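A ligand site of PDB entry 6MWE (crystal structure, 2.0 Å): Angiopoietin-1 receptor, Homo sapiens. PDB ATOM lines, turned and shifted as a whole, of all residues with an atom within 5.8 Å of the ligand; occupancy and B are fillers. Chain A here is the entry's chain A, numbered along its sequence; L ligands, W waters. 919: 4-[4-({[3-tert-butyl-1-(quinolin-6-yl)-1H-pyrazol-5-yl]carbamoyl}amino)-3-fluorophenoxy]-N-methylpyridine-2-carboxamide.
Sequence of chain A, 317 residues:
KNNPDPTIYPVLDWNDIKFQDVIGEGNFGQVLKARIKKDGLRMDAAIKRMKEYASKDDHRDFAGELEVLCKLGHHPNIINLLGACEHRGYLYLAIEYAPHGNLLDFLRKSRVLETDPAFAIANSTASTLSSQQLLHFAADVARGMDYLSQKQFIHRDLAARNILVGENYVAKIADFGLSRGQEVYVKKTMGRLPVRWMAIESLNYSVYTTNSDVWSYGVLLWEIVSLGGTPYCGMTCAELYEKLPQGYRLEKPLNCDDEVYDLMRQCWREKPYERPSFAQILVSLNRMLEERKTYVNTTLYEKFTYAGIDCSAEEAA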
ATOM      1  N   ILE A  23       7.955   5.210   4.335  1.00  0.00           N
ATOM      2  CA  ILE A  23       8.993   6.163   4.783  1.00  0.00           C
ATOM      3  C   ILE A  23      10.119   5.485   5.554  1.00  0.00           C
ATOM      4  O   ILE A  23      10.872   6.126   6.326  1.00  0.00           O
ATOM      5  CB  ILE A  23       8.390   7.274   5.673  1.00  0.00           C
ATOM      6  CG1 ILE A  23       7.520   6.665   6.806  1.00  0.00           C
ATOM      7  CG2 ILE A  23       7.586   8.234   4.835  1.00  0.00           C
ATOM      8  CD1 ILE A  23       6.890   7.693   7.732  1.00  0.00           C
ATOM      9  N   VAL A  31       7.531   1.109   7.638  1.00  0.00           N
ATOM     10  CA  VAL A  31       6.884   2.229   8.277  1.00  0.00           C
ATOM     11  C   VAL A  31       6.241   3.069   7.173  1.00  0.00           C
ATOM     12  O   VAL A  31       6.892   3.369   6.173  1.00  0.00           O
ATOM     13  CB  VAL A  31       7.896   3.026   9.106  1.00  0.00           C
ATOM     14  CG1 VAL A  31       7.289   4.325   9.642  1.00  0.00           C
ATOM     15  CG2 VAL A  31       8.407   2.156  10.281  1.00  0.00           C
ATOM     16  N   ALA A  46       2.761   7.787  11.796  1.00  0.00           N
ATOM     17  CA  ALA A  46       3.664   6.864  11.141  1.00  0.00           C
ATOM     18  C   ALA A  46       3.277   5.473  11.605  1.00  0.00           C
ATOM     19  O   ALA A  46       3.264   5.218  12.809  1.00  0.00           O
ATOM     20  CB  ALA A  46       5.114   7.163  11.508  1.00  0.00           C
ATOM     21  N   LYS A  48       3.894   1.471  11.851  1.00  0.00           N
ATOM     22  CA  LYS A  48       4.839   0.386  11.712  1.00  0.00           C
ATOM     23  C   LYS A  48       4.050  -0.898  11.490  1.00  0.00           C
ATOM     24  O   LYS A  48       3.218  -1.264  12.318  1.00  0.00           O
ATOM     25  CB  LYS A  48       5.684   0.245  12.969  1.00  0.00           C
ATOM     26  CG  LYS A  48       6.863  -0.709  12.801  1.00  0.00           C
ATOM     27  CD  LYS A  48       7.840  -0.586  13.949  1.00  0.00           C
ATOM     28  CE  LYS A  48       8.931  -1.620  13.804  1.00  0.00           C
ATOM     29  NZ  LYS A  48       9.693  -1.738  15.059  1.00  0.00           N
ATOM     30  N   GLY A  64       5.352  -5.931  22.976  1.00  0.00           N
ATOM     31  CA  GLY A  64       6.714  -5.531  23.331  1.00  0.00           C
ATOM     32  C   GLY A  64       6.961  -4.048  23.069  1.00  0.00           C
ATOM     33  O   GLY A  64       6.956  -3.219  23.979  1.00  0.00           O
ATOM     34  N   GLU A  65       7.188  -3.703  21.803  1.00  0.00           N
ATOM     35  CA  GLU A  65       7.281  -2.303  21.400  1.00  0.00           C
ATOM     36  C   GLU A  65       5.978  -1.580  21.802  1.00  0.00           C
ATOM     37  O   GLU A  65       5.999  -0.413  22.295  1.00  0.00           O
ATOM     38  CB  GLU A  65       7.536  -2.190  19.884  1.00  0.00           C
ATOM     39  CG  GLU A  65       7.844  -0.739  19.467  1.00  0.00           C
ATOM     40  CD  GLU A  65       8.448  -0.573  18.068  1.00  0.00           C
ATOM     41  OE1 GLU A  65       8.741   0.606  17.721  1.00  0.00           O
ATOM     42  OE2 GLU A  65       8.589  -1.551  17.273  1.00  0.00           O
ATOM     43  N   VAL A  68       5.966  -0.852  25.736  1.00  0.00           N
ATOM     44  CA  VAL A  68       6.912   0.212  26.040  1.00  0.00           C
ATOM     45  C   VAL A  68       6.354   1.590  25.644  1.00  0.00           C
ATOM     46  O   VAL A  68       6.436   2.552  26.418  1.00  0.00           O
ATOM     47  CB  VAL A  68       8.283  -0.034  25.363  1.00  0.00           C
ATOM     48  CG1 VAL A  68       9.228   1.118  25.666  1.00  0.00           C
ATOM     49  CG2 VAL A  68       8.906  -1.322  25.898  1.00  0.00           C
ATOM     50  N   LEU A  69       5.834   1.689  24.432  1.00  0.00           N
ATOM     51  CA  LEU A  69       5.268   2.944  23.938  1.00  0.00           C
ATOM     52  C   LEU A  69       4.006   3.331  24.723  1.00  0.00           C
ATOM     53  O   LEU A  69       3.789   4.497  25.013  1.00  0.00           O
ATOM     54  CB  LEU A  69       5.003   2.858  22.436  1.00  0.00           C
ATOM     55  CG  LEU A  69       6.264   2.800  21.555  1.00  0.00           C
ATOM     56  CD1 LEU A  69       5.923   2.588  20.098  1.00  0.00           C
ATOM     57  CD2 LEU A  69       7.058   4.070  21.718  1.00  0.00           C
ATOM     58  N   LEU A  72       5.376   4.823  28.216  1.00  0.00           N
ATOM     59  CA  LEU A  72       6.217   6.029  28.224  1.00  0.00           C
ATOM     60  C   LEU A  72       5.786   7.116  27.263  1.00  0.00           C
ATOM     61  O   LEU A  72       6.220   8.274  27.402  1.00  0.00           O
ATOM     62  CB  LEU A  72       7.656   5.637  27.907  1.00  0.00           C
ATOM     63  CG  LEU A  72       8.340   4.617  28.836  1.00  0.00           C
ATOM     64  CD1 LEU A  72       9.688   4.254  28.259  1.00  0.00           C
ATOM     65  CD2 LEU A  72       8.496   5.157  30.239  1.00  0.00           C
ATOM     66  N   ILE A  78       8.972  11.807  24.571  1.00  0.00           N
ATOM     67  CA  ILE A  78       9.054  10.367  24.162  1.00  0.00           C
ATOM     68  C   ILE A  78       8.010  10.134  23.083  1.00  0.00           C
ATOM     69  O   ILE A  78       6.857  10.552  23.225  1.00  0.00           O
ATOM     70  CB  ILE A  78       8.808   9.432  25.328  1.00  0.00           C
ATOM     71  CG1 ILE A  78       9.904   9.711  26.414  1.00  0.00           C
ATOM     72  CG2 ILE A  78       8.868   7.970  24.874  1.00  0.00           C
ATOM     73  CD1 ILE A  78       9.879   8.818  27.610  1.00  0.00           C
ATOM     74  N   ILE A  79       8.421   9.519  21.969  1.00  0.00           N
ATOM     75  CA  ILE A  79       7.502   9.370  20.829  1.00  0.00           C
ATOM     76  C   ILE A  79       6.317   8.520  21.306  1.00  0.00           C
ATOM     77  O   ILE A  79       6.493   7.547  22.088  1.00  0.00           O
ATOM     78  CB  ILE A  79       8.246   8.792  19.584  1.00  0.00           C
ATOM     79  CG1 ILE A  79       7.446   9.091  18.308  1.00  0.00           C
ATOM     80  CG2 ILE A  79       8.534   7.308  19.758  1.00  0.00           C
ATOM     81  CD1 ILE A  79       7.410  10.560  17.959  1.00  0.00           C
ATOM     82  N   LEU A  93       1.284  -0.665  14.350  1.00  0.00           N
ATOM     83  CA  LEU A  93       1.427   0.299  15.436  1.00  0.00           C
ATOM     84  C   LEU A  93       1.394   1.705  14.847  1.00  0.00           C
ATOM     85  O   LEU A  93       2.255   2.045  14.046  1.00  0.00           O
ATOM     86  CB  LEU A  93       2.754   0.081  16.186  1.00  0.00           C
ATOM     87  CG  LEU A  93       2.942  -1.175  17.061  1.00  0.00           C
ATOM     88  CD1 LEU A  93       4.178  -0.994  17.890  1.00  0.00           C
ATOM     89  CD2 LEU A  93       1.750  -1.457  17.960  1.00  0.00           C
ATOM     90  N   ILE A  95       2.105   5.421  15.256  1.00  0.00           N
ATOM     91  CA  ILE A  95       3.069   6.164  16.073  1.00  0.00           C
ATOM     92  C   ILE A  95       2.894   7.644  15.761  1.00  0.00           C
ATOM     93  O   ILE A  95       2.612   8.010  14.614  1.00  0.00           O
ATOM     94  CB  ILE A  95       4.523   5.753  15.759  1.00  0.00           C
ATOM     95  CG1 ILE A  95       4.734   4.246  15.863  1.00  0.00           C
ATOM     96  CG2 ILE A  95       5.529   6.496  16.610  1.00  0.00           C
ATOM     97  CD1 ILE A  95       4.536   3.687  17.223  1.00  0.00           C
ATOM     98  N   GLU A  96       3.056   8.468  16.780  1.00  0.00           N
ATOM     99  CA  GLU A  96       3.015   9.906  16.655  1.00  0.00           C
ATOM    100  C   GLU A  96       3.894  10.309  15.494  1.00  0.00           C
ATOM    101  O   GLU A  96       5.045   9.891  15.438  1.00  0.00           O
ATOM    102  CB  GLU A  96       3.556  10.511  17.945  1.00  0.00           C
ATOM    103  CG  GLU A  96       3.614  12.036  18.039  1.00  0.00           C
ATOM    104  CD  GLU A  96       4.256  12.495  19.364  1.00  0.00           C
ATOM    105  OE1 GLU A  96       4.656  11.638  20.202  1.00  0.00           O
ATOM    106  OE2 GLU A  96       4.383  13.687  19.553  1.00  0.00           O
ATOM    107  N   TYR A  97       3.346  11.125  14.581  1.00  0.00           N
ATOM    108  CA  TYR A  97       4.127  11.584  13.435  1.00  0.00           C
ATOM    109  C   TYR A  97       5.010  12.788  13.833  1.00  0.00           C
ATOM    110  O   TYR A  97       4.549  13.693  14.505  1.00  0.00           O
ATOM    111  CB  TYR A  97       3.203  11.936  12.266  1.00  0.00           C
ATOM    112  CG  TYR A  97       3.941  12.263  11.008  1.00  0.00           C
ATOM    113  CD1 TYR A  97       4.641  11.284  10.342  1.00  0.00           C
ATOM    114  CD2 TYR A  97       3.951  13.562  10.492  1.00  0.00           C
ATOM    115  CE1 TYR A  97       5.316  11.557   9.192  1.00  0.00           C
ATOM    116  CE2 TYR A  97       4.632  13.851   9.318  1.00  0.00           C
ATOM    117  CZ  TYR A  97       5.315  12.848   8.680  1.00  0.00           C
ATOM    118  OH  TYR A  97       5.982  13.086   7.518  1.00  0.00           O
ATOM    119  N   ALA A  98       6.271  12.778  13.440  1.00  0.00           N
ATOM    120  CA  ALA A  98       7.187  13.880  13.739  1.00  0.00           C
ATOM    121  C   ALA A  98       7.514  14.553  12.400  1.00  0.00           C
ATOM    122  O   ALA A  98       8.343  14.054  11.660  1.00  0.00           O
ATOM    123  CB  ALA A  98       8.462  13.339  14.355  1.00  0.00           C
ATOM    124  N   PRO A  99       6.863  15.706  12.100  1.00  0.00           N
ATOM    125  CA  PRO A  99       6.981  16.226  10.719  1.00  0.00           C
ATOM    126  C   PRO A  99       8.374  16.593  10.281  1.00  0.00           C
ATOM    127  O   PRO A  99       8.641  16.616   9.065  1.00  0.00           O
ATOM    128  CB  PRO A  99       6.082  17.492  10.710  1.00  0.00           C
ATOM    129  CG  PRO A  99       5.269  17.451  11.973  1.00  0.00           C
ATOM    130  CD  PRO A  99       5.963  16.501  12.940  1.00  0.00           C
ATOM    131  N   HIS A 100       9.262  16.933  11.212  1.00  0.00           N
ATOM    132  CA  HIS A 100      10.589  17.405  10.843  1.00  0.00           C
ATOM    133  C   HIS A 100      11.645  16.296  10.775  1.00  0.00           C
ATOM    134  O   HIS A 100      12.782  16.568  10.483  1.00  0.00           O
ATOM    135  CB  HIS A 100      11.002  18.547  11.781  1.00  0.00           C
ATOM    136  CG  HIS A 100       9.973  19.606  11.871  1.00  0.00           C
ATOM    137  ND1 HIS A 100       9.709  20.474  10.824  1.00  0.00           N
ATOM    138  CD2 HIS A 100       9.056  19.890  12.826  1.00  0.00           C
ATOM    139  CE1 HIS A 100       8.714  21.257  11.141  1.00  0.00           C
ATOM    140  NE2 HIS A 100       8.292  20.936  12.353  1.00  0.00           N
ATOM    141  N   GLY A 101      11.251  15.043  11.035  1.00  0.00           N
ATOM    142  CA  GLY A 101      12.185  13.907  10.846  1.00  0.00           C
ATOM    143  C   GLY A 101      13.213  13.799  11.960  1.00  0.00           C
ATOM    144  O   GLY A 101      13.050  14.400  13.047  1.00  0.00           O
ATOM    145  N   ASN A 102      14.271  13.019  11.734  1.00  0.00           N
ATOM    146  CA  ASN A 102      15.222  12.725  12.801  1.00  0.00           C
ATOM    147  C   ASN A 102      16.170  13.915  13.019  1.00  0.00           C
ATOM    148  O   ASN A 102      16.451  14.700  12.079  1.00  0.00           O
ATOM    149  CB  ASN A 102      15.976  11.411  12.485  1.00  0.00           C
ATOM    150  CG  ASN A 102      17.081  11.588  11.431  1.00  0.00           C
ATOM    151  OD1 ASN A 102      18.157  12.071  11.727  1.00  0.00           O
ATOM    152  ND2 ASN A 102      16.846  11.131  10.276  1.00  0.00           N
ATOM    153  N   LEU A 148      12.234   8.391  31.476  1.00  0.00           N
ATOM    154  CA  LEU A 148      12.494   7.055  31.080  1.00  0.00           C
ATOM    155  C   LEU A 148      13.397   6.328  32.099  1.00  0.00           C
ATOM    156  O   LEU A 148      13.093   5.172  32.485  1.00  0.00           O
ATOM    157  CB  LEU A 148      13.034   7.086  29.623  1.00  0.00           C
ATOM    158  CG  LEU A 148      13.579   5.981  28.761  1.00  0.00           C
ATOM    159  CD1 LEU A 148      13.744   6.493  27.324  1.00  0.00           C
ATOM    160  CD2 LEU A 148      14.900   5.408  29.231  1.00  0.00           C
ATOM    161  N   PHE A 153      13.858   2.197  32.591  1.00  0.00           N
ATOM    162  CA  PHE A 153      14.246   1.777  31.247  1.00  0.00           C
ATOM    163  C   PHE A 153      15.685   2.198  31.017  1.00  0.00           C
ATOM    164  O   PHE A 153      16.125   3.199  31.569  1.00  0.00           O
ATOM    165  CB  PHE A 153      13.289   2.339  30.164  1.00  0.00           C
ATOM    166  CG  PHE A 153      11.932   1.687  30.145  1.00  0.00           C
ATOM    167  CD1 PHE A 153      10.945   2.103  31.027  1.00  0.00           C
ATOM    168  CD2 PHE A 153      11.648   0.633  29.273  1.00  0.00           C
ATOM    169  CE1 PHE A 153       9.697   1.461  31.063  1.00  0.00           C
ATOM    170  CE2 PHE A 153      10.413   0.003  29.297  1.00  0.00           C
ATOM    171  CZ  PHE A 153       9.438   0.407  30.210  1.00  0.00           C
ATOM    172  N   HIS A 155      18.035   2.915  27.625  1.00  0.00           N
ATOM    173  CA  HIS A 155      17.852   3.075  26.200  1.00  0.00           C
ATOM    174  C   HIS A 155      18.821   2.206  25.375  1.00  0.00           C
ATOM    175  O   HIS A 155      18.383   1.446  24.533  1.00  0.00           O
ATOM    176  CB  HIS A 155      17.936   4.543  25.804  1.00  0.00           C
ATOM    177  CG  HIS A 155      17.446   4.806  24.416  1.00  0.00           C
ATOM    178  ND1 HIS A 155      18.170   4.445  23.301  1.00  0.00           N
ATOM    179  CD2 HIS A 155      16.335   5.450  23.957  1.00  0.00           C
ATOM    180  CE1 HIS A 155      17.499   4.798  22.216  1.00  0.00           C
ATOM    181  NE2 HIS A 155      16.396   5.433  22.591  1.00  0.00           N
ATOM    182  N   LEU A 164      13.553  12.294  17.285  1.00  0.00           N
ATOM    183  CA  LEU A 164      12.655  12.873  16.289  1.00  0.00           C
ATOM    184  C   LEU A 164      12.345  14.326  16.655  1.00  0.00           C
ATOM    185  O   LEU A 164      12.243  14.684  17.825  1.00  0.00           O
ATOM    186  CB  LEU A 164      11.384  12.039  16.203  1.00  0.00           C
ATOM    187  CG  LEU A 164      11.627  10.694  15.501  1.00  0.00           C
ATOM    188  CD1 LEU A 164      10.476   9.755  15.703  1.00  0.00           C
ATOM    189  CD2 LEU A 164      11.899  10.894  14.023  1.00  0.00           C
ATOM    190  N   ILE A 173      12.247  11.227  21.987  1.00  0.00           N
ATOM    191  CA  ILE A 173      13.144  10.094  22.025  1.00  0.00           C
ATOM    192  C   ILE A 173      12.470   8.900  21.325  1.00  0.00           C
ATOM    193  O   ILE A 173      11.298   8.588  21.593  1.00  0.00           O
ATOM    194  CB  ILE A 173      13.593   9.747  23.458  1.00  0.00           C
ATOM    195  CG1 ILE A 173      14.378  10.924  24.061  1.00  0.00           C
ATOM    196  CG2 ILE A 173      14.451   8.492  23.478  1.00  0.00           C
ATOM    197  CD1 ILE A 173      14.405  10.889  25.572  1.00  0.00           C
ATOM    198  N   ALA A 174      13.222   8.209  20.485  1.00  0.00           N
ATOM    199  CA  ALA A 174      12.692   7.066  19.754  1.00  0.00           C
ATOM    200  C   ALA A 174      13.728   5.947  19.687  1.00  0.00           C
ATOM    201  O   ALA A 174      14.853   6.085  20.189  1.00  0.00           O
ATOM    202  CB  ALA A 174      12.270   7.508  18.331  1.00  0.00           C
ATOM    203  N   ASP A 175      13.368   4.842  19.058  1.00  0.00           N
ATOM    204  CA  ASP A 175      14.298   3.715  18.849  1.00  0.00           C
ATOM    205  C   ASP A 175      13.808   2.949  17.645  1.00  0.00           C
ATOM    206  O   ASP A 175      12.672   2.579  17.561  1.00  0.00           O
ATOM    207  CB  ASP A 175      14.332   2.820  20.120  1.00  0.00           C
ATOM    208  CG  ASP A 175      15.331   1.661  20.004  1.00  0.00           C
ATOM    209  OD1 ASP A 175      15.527   1.116  18.912  1.00  0.00           O
ATOM    210  OD2 ASP A 175      15.829   1.201  21.062  1.00  0.00           O
ATOM    211  N   PHE A 176      14.667   2.823  16.649  1.00  0.00           N
ATOM    212  CA  PHE A 176      14.257   2.363  15.328  1.00  0.00           C
ATOM    213  C   PHE A 176      14.615   0.881  15.163  1.00  0.00           C
ATOM    214  O   PHE A 176      14.490   0.313  14.056  1.00  0.00           O
ATOM    215  CB  PHE A 176      14.879   3.245  14.225  1.00  0.00           C
ATOM    216  CG  PHE A 176      14.174   4.592  14.044  1.00  0.00           C
ATOM    217  CD1 PHE A 176      12.964   4.656  13.377  1.00  0.00           C
ATOM    218  CD2 PHE A 176      14.701   5.744  14.558  1.00  0.00           C
ATOM    219  CE1 PHE A 176      12.311   5.872  13.205  1.00  0.00           C
ATOM    220  CE2 PHE A 176      14.064   6.959  14.402  1.00  0.00           C
ATOM    221  CZ  PHE A 176      12.854   7.024  13.735  1.00  0.00           C
ATOM    222  N   GLY A 177      14.993   0.247  16.272  1.00  0.00           N
ATOM    223  CA  GLY A 177      15.105  -1.197  16.335  1.00  0.00           C
ATOM    224  C   GLY A 177      16.464  -1.788  16.013  1.00  0.00           C
ATOM    225  O   GLY A 177      16.633  -3.029  16.054  1.00  0.00           O
ATOM    226  N   ARG A 180      18.160  -4.217  18.395  1.00  0.00           N
ATOM    227  CA  ARG A 180      17.494  -5.514  18.477  1.00  0.00           C
ATOM    228  C   ARG A 180      17.597  -6.289  17.159  1.00  0.00           C
ATOM    229  O   ARG A 180      16.907  -7.283  16.974  1.00  0.00           O
ATOM    230  CB  ARG A 180      16.035  -5.335  18.842  1.00  0.00           C
ATOM    231  CG  ARG A 180      15.807  -4.714  20.212  1.00  0.00           C
ATOM    232  CD  ARG A 180      14.317  -4.589  20.494  1.00  0.00           C
ATOM    233  NE  ARG A 180      14.030  -4.157  21.882  1.00  0.00           N
ATOM    234  CZ  ARG A 180      14.054  -2.890  22.333  1.00  0.00           C
ATOM    235  NH1 ARG A 180      13.768  -2.653  23.624  1.00  0.00           N
ATOM    236  NH2 ARG A 180      14.371  -1.869  21.538  1.00  0.00           N
ATOM    237  N   GLN A 182      16.680  -5.291  14.336  1.00  0.00           N
ATOM    238  CA  GLN A 182      15.391  -5.159  13.659  1.00  0.00           C
ATOM    239  C   GLN A 182      15.178  -3.762  13.109  1.00  0.00           C
ATOM    240  O   GLN A 182      14.075  -3.239  13.199  1.00  0.00           O
ATOM    241  CB  GLN A 182      14.231  -5.432  14.635  1.00  0.00           C
ATOM    242  CG  GLN A 182      14.267  -6.777  15.315  1.00  0.00           C
ATOM    243  CD  GLN A 182      12.996  -7.043  16.097  1.00  0.00           C
ATOM    244  OE1 GLN A 182      11.979  -6.398  15.870  1.00  0.00           O
ATOM    245  NE2 GLN A 182      13.055  -7.984  17.009  1.00  0.00           N
ATOM    246  N   VAL A 184      14.456  -0.371  11.189  1.00  0.00           N
ATOM    247  CA  VAL A 184      13.690   0.277  10.098  1.00  0.00           C
ATOM    248  C   VAL A 184      14.314   1.614   9.603  1.00  0.00           C
ATOM    249  O   VAL A 184      14.523   2.546  10.385  1.00  0.00           O
ATOM    250  CB  VAL A 184      12.202   0.533  10.459  1.00  0.00           C
ATOM    251  CG1 VAL A 184      11.468  -0.786  10.695  1.00  0.00           C
ATOM    252  CG2 VAL A 184      12.051   1.500  11.639  1.00  0.00           C
HETATM  253  C1  919 L   1      11.099   0.233  20.835  1.00  0.00           C
HETATM  254  C2  919 L   1      10.743  -0.771  21.744  1.00  0.00           C
HETATM  255  C3  919 L   1      10.809  -2.109  21.363  1.00  0.00           C
HETATM  256  C4  919 L   1      11.229  -2.449  20.081  1.00  0.00           C
HETATM  257  C5  919 L   1      11.596  -1.457  19.180  1.00  0.00           C
HETATM  258  C6  919 L   1      11.537  -0.102  19.561  1.00  0.00           C
HETATM  259  C9  919 L   1      11.696  -4.127  18.489  1.00  0.00           C
HETATM  260  N10 919 L   1      11.277  -3.762  19.727  1.00  0.00           N
HETATM  261  C13 919 L   1      12.026  -1.808  17.906  1.00  0.00           C
HETATM  262  C14 919 L   1      12.063  -3.165  17.554  1.00  0.00           C
HETATM  263  C22 919 L   1       7.430   9.599  13.387  1.00  0.00           C
HETATM  264  N23 919 L   1       7.893  10.273  12.315  1.00  0.00           N
HETATM  265  C24 919 L   1       8.582   9.617  11.336  1.00  0.00           C
HETATM  266  C25 919 L   1       8.834   8.256  11.439  1.00  0.00           C
HETATM  267  C26 919 L   1       8.398   7.551  12.545  1.00  0.00           C
HETATM  268  C27 919 L   1       7.673   8.229  13.519  1.00  0.00           C
HETATM  269  C34 919 L   1       9.654   5.345  16.088  1.00  0.00           C
HETATM  270  C35 919 L   1       9.510   6.067  14.896  1.00  0.00           C
HETATM  271  C36 919 L   1       8.830   5.522  13.800  1.00  0.00           C
HETATM  272  C37 919 L   1       8.298   4.260  13.912  1.00  0.00           C
HETATM  273  C38 919 L   1       8.439   3.534  15.088  1.00  0.00           C
HETATM  274  C39 919 L   1       9.110   4.057  16.193  1.00  0.00           C
HETATM  275  C46 919 L   1      11.262   3.291  22.542  1.00  0.00           C
HETATM  276  C47 919 L   1      10.719   3.709  21.321  1.00  0.00           C
HETATM  277  C48 919 L   1      10.598   2.576  20.507  1.00  0.00           C
HETATM  278  N49 919 L   1      11.041   1.518  21.230  1.00  0.00           N
HETATM  279  N50 919 L   1      11.437   1.960  22.462  1.00  0.00           N
HETATM  280  N56 919 L   1      10.107   2.486  19.234  1.00  0.00           N
HETATM  281  C58 919 L   1       9.967   3.531  18.399  1.00  0.00           C
HETATM  282  N60 919 L   1       9.194   3.280  17.321  1.00  0.00           N
HETATM  283  O63 919 L   1      10.494   4.623  18.625  1.00  0.00           O
HETATM  284  O65 919 L   1       8.674   6.198  12.610  1.00  0.00           O
HETATM  285  F68 919 L   1       7.905   2.311  15.153  1.00  0.00           F
HETATM  286  C70 919 L   1       9.081  10.327  10.124  1.00  0.00           C
HETATM  287  O72 919 L   1       9.546   9.642   9.222  1.00  0.00           O
HETATM  288  N74 919 L   1       9.064  11.647  10.096  1.00  0.00           N
HETATM  289  C76 919 L   1       9.531  12.395   8.941  1.00  0.00           C
HETATM  290  C79 919 L   1      11.573   4.143  23.750  1.00  0.00           C
HETATM  291  C81 919 L   1      12.620   5.185  23.410  1.00  0.00           C
HETATM  292  C83 919 L   1      10.272   4.814  24.178  1.00  0.00           C
HETATM  293  C85 919 L   1      12.081   3.255  24.889  1.00  0.00           C
HETATM  294  O   HOH W   1      11.076   0.972  15.898  1.00  0.00           O
HETATM  295  O   HOH W   2      10.345  -6.089  21.521  1.00  0.00           O
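OE1 of Glu 65 is in hydrogen-bond range of N60 of the ligand (2.7 Å). O of Ala 98 is in hydrogen-bond range of N74 of the ligand (3.0 Å). The backbone carbonyl oxygen (O) of Asp 175 lies close to a nitrogen (N56) of the ligand (3.1 Å). N of Ala 98 sits at hydrogen-bond distance from N23 of the ligand. O63 of the ligand sits at hydrogen-bond distance from N of Asp 175 (2.9 Å).
The backbone NH (N) of Ile 95 is in hydrogen-bond range of the backbone carbonyl oxygen (O) of Ala 46. The guanidinium group (NH2) of Arg 180 lies within salt-bridge range of the side-chain carboxylate (OD2) of Asp 175 (3.4 Å). The backbone carbonyl oxygen (O) of Val 31 is in hydrogen-bond range of the backbone NH (N) of Ile 23, at 2.8 Å. The backbone carbonyl oxygen (O) of Ala 174 is in hydrogen-bond range of a ring nitrogen (NE2) of His 155 (2.9 Å). N of Gln 182 is in hydrogen-bond range of O of Gly 177 (2.8 Å). The side-chain amino group (NZ) of Lys 48 lies within salt-bridge range of the side-chain carboxylate (OE2) of Glu 65. The backbone NH (N) of Val 184 sits at hydrogen-bond distance from the backbone carbonyl oxygen (O) of Phe 176 (2.9 Å). The backbone carbonyl oxygen of Ile 173 sits at hydrogen-bond distance from the backbone NH of Ile 79.
CD1 of Ile 23 touches O72 of the ligand, at 3.6 Å. Val 31 touches the ligand (CG1 to O65, 3.8 Å). CB of Ala 46 touches C27 of the ligand (3.4 Å). Lys 48 touches the ligand. Val 68 touches the ligand (CG1 to C85, 3.6 Å). Leu 69 touches the ligand. Ile 78 touches the ligand (CG2 to C83, 3.5 Å). Ile 79 touches the ligand. Ile 95 touches the ligand (CG1 to F68, 3.8 Å). O of Glu 96 touches C22 of the ligand, 3.2 Å away. CA of Tyr 97 touches C22 of the ligand (3.9 Å). Gly 101 touches the ligand. His 155 touches the ligand (CD2 to C81, 3.8 Å). Leu 164 touches the ligand. Ile 173 touches the ligand. Ala 174 touches the ligand (CB to O63, 3.4 Å). CE1 of Phe 176 touches C35 of the ligand, at 3.3 Å. Gly 177 touches the ligand (CA to C13, 3.5 Å). Arg 180 touches the ligand. Gln 182 touches the ligand (OE1 to C9, 3.5 Å). Hydrophobic or aromatic side chains that line the ligand: Ile 23, Val 31, Ala 46, Val 68, Leu 69, Ile 78, Ile 79, Ile 95, Tyr 97, Ala 98, His 155, Leu 164, Ile 173, Ala 174 and Phe 176. Within 4 Å of the ligand: Ile 23, Val 31, Ala 46, Lys 48, Glu 65, Val 68, Leu 69, Ile 78, Ile 79, Ile 95, Glu 96, Tyr 97, Ala 98, Gly 101, His 155, Leu 164, Ile 173, Ala 174, Asp 175, Phe 176, Gly 177, Arg 180 and Gln 182. Along chain A the residues within 4 Å of the ligand span positions 23 to 182. The nearest printed residue that does not touch the ligand is Leu 72 (4.2 Å).
Water W1 lies within hydrogen-bond range of the backbone carbonyl oxygen (O) of Asp 175, the side-chain carboxylate (OE1) of Glu 65, the side-chain amino group (NZ) of Lys 48 and a nitrogen (N60) of the ligand.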
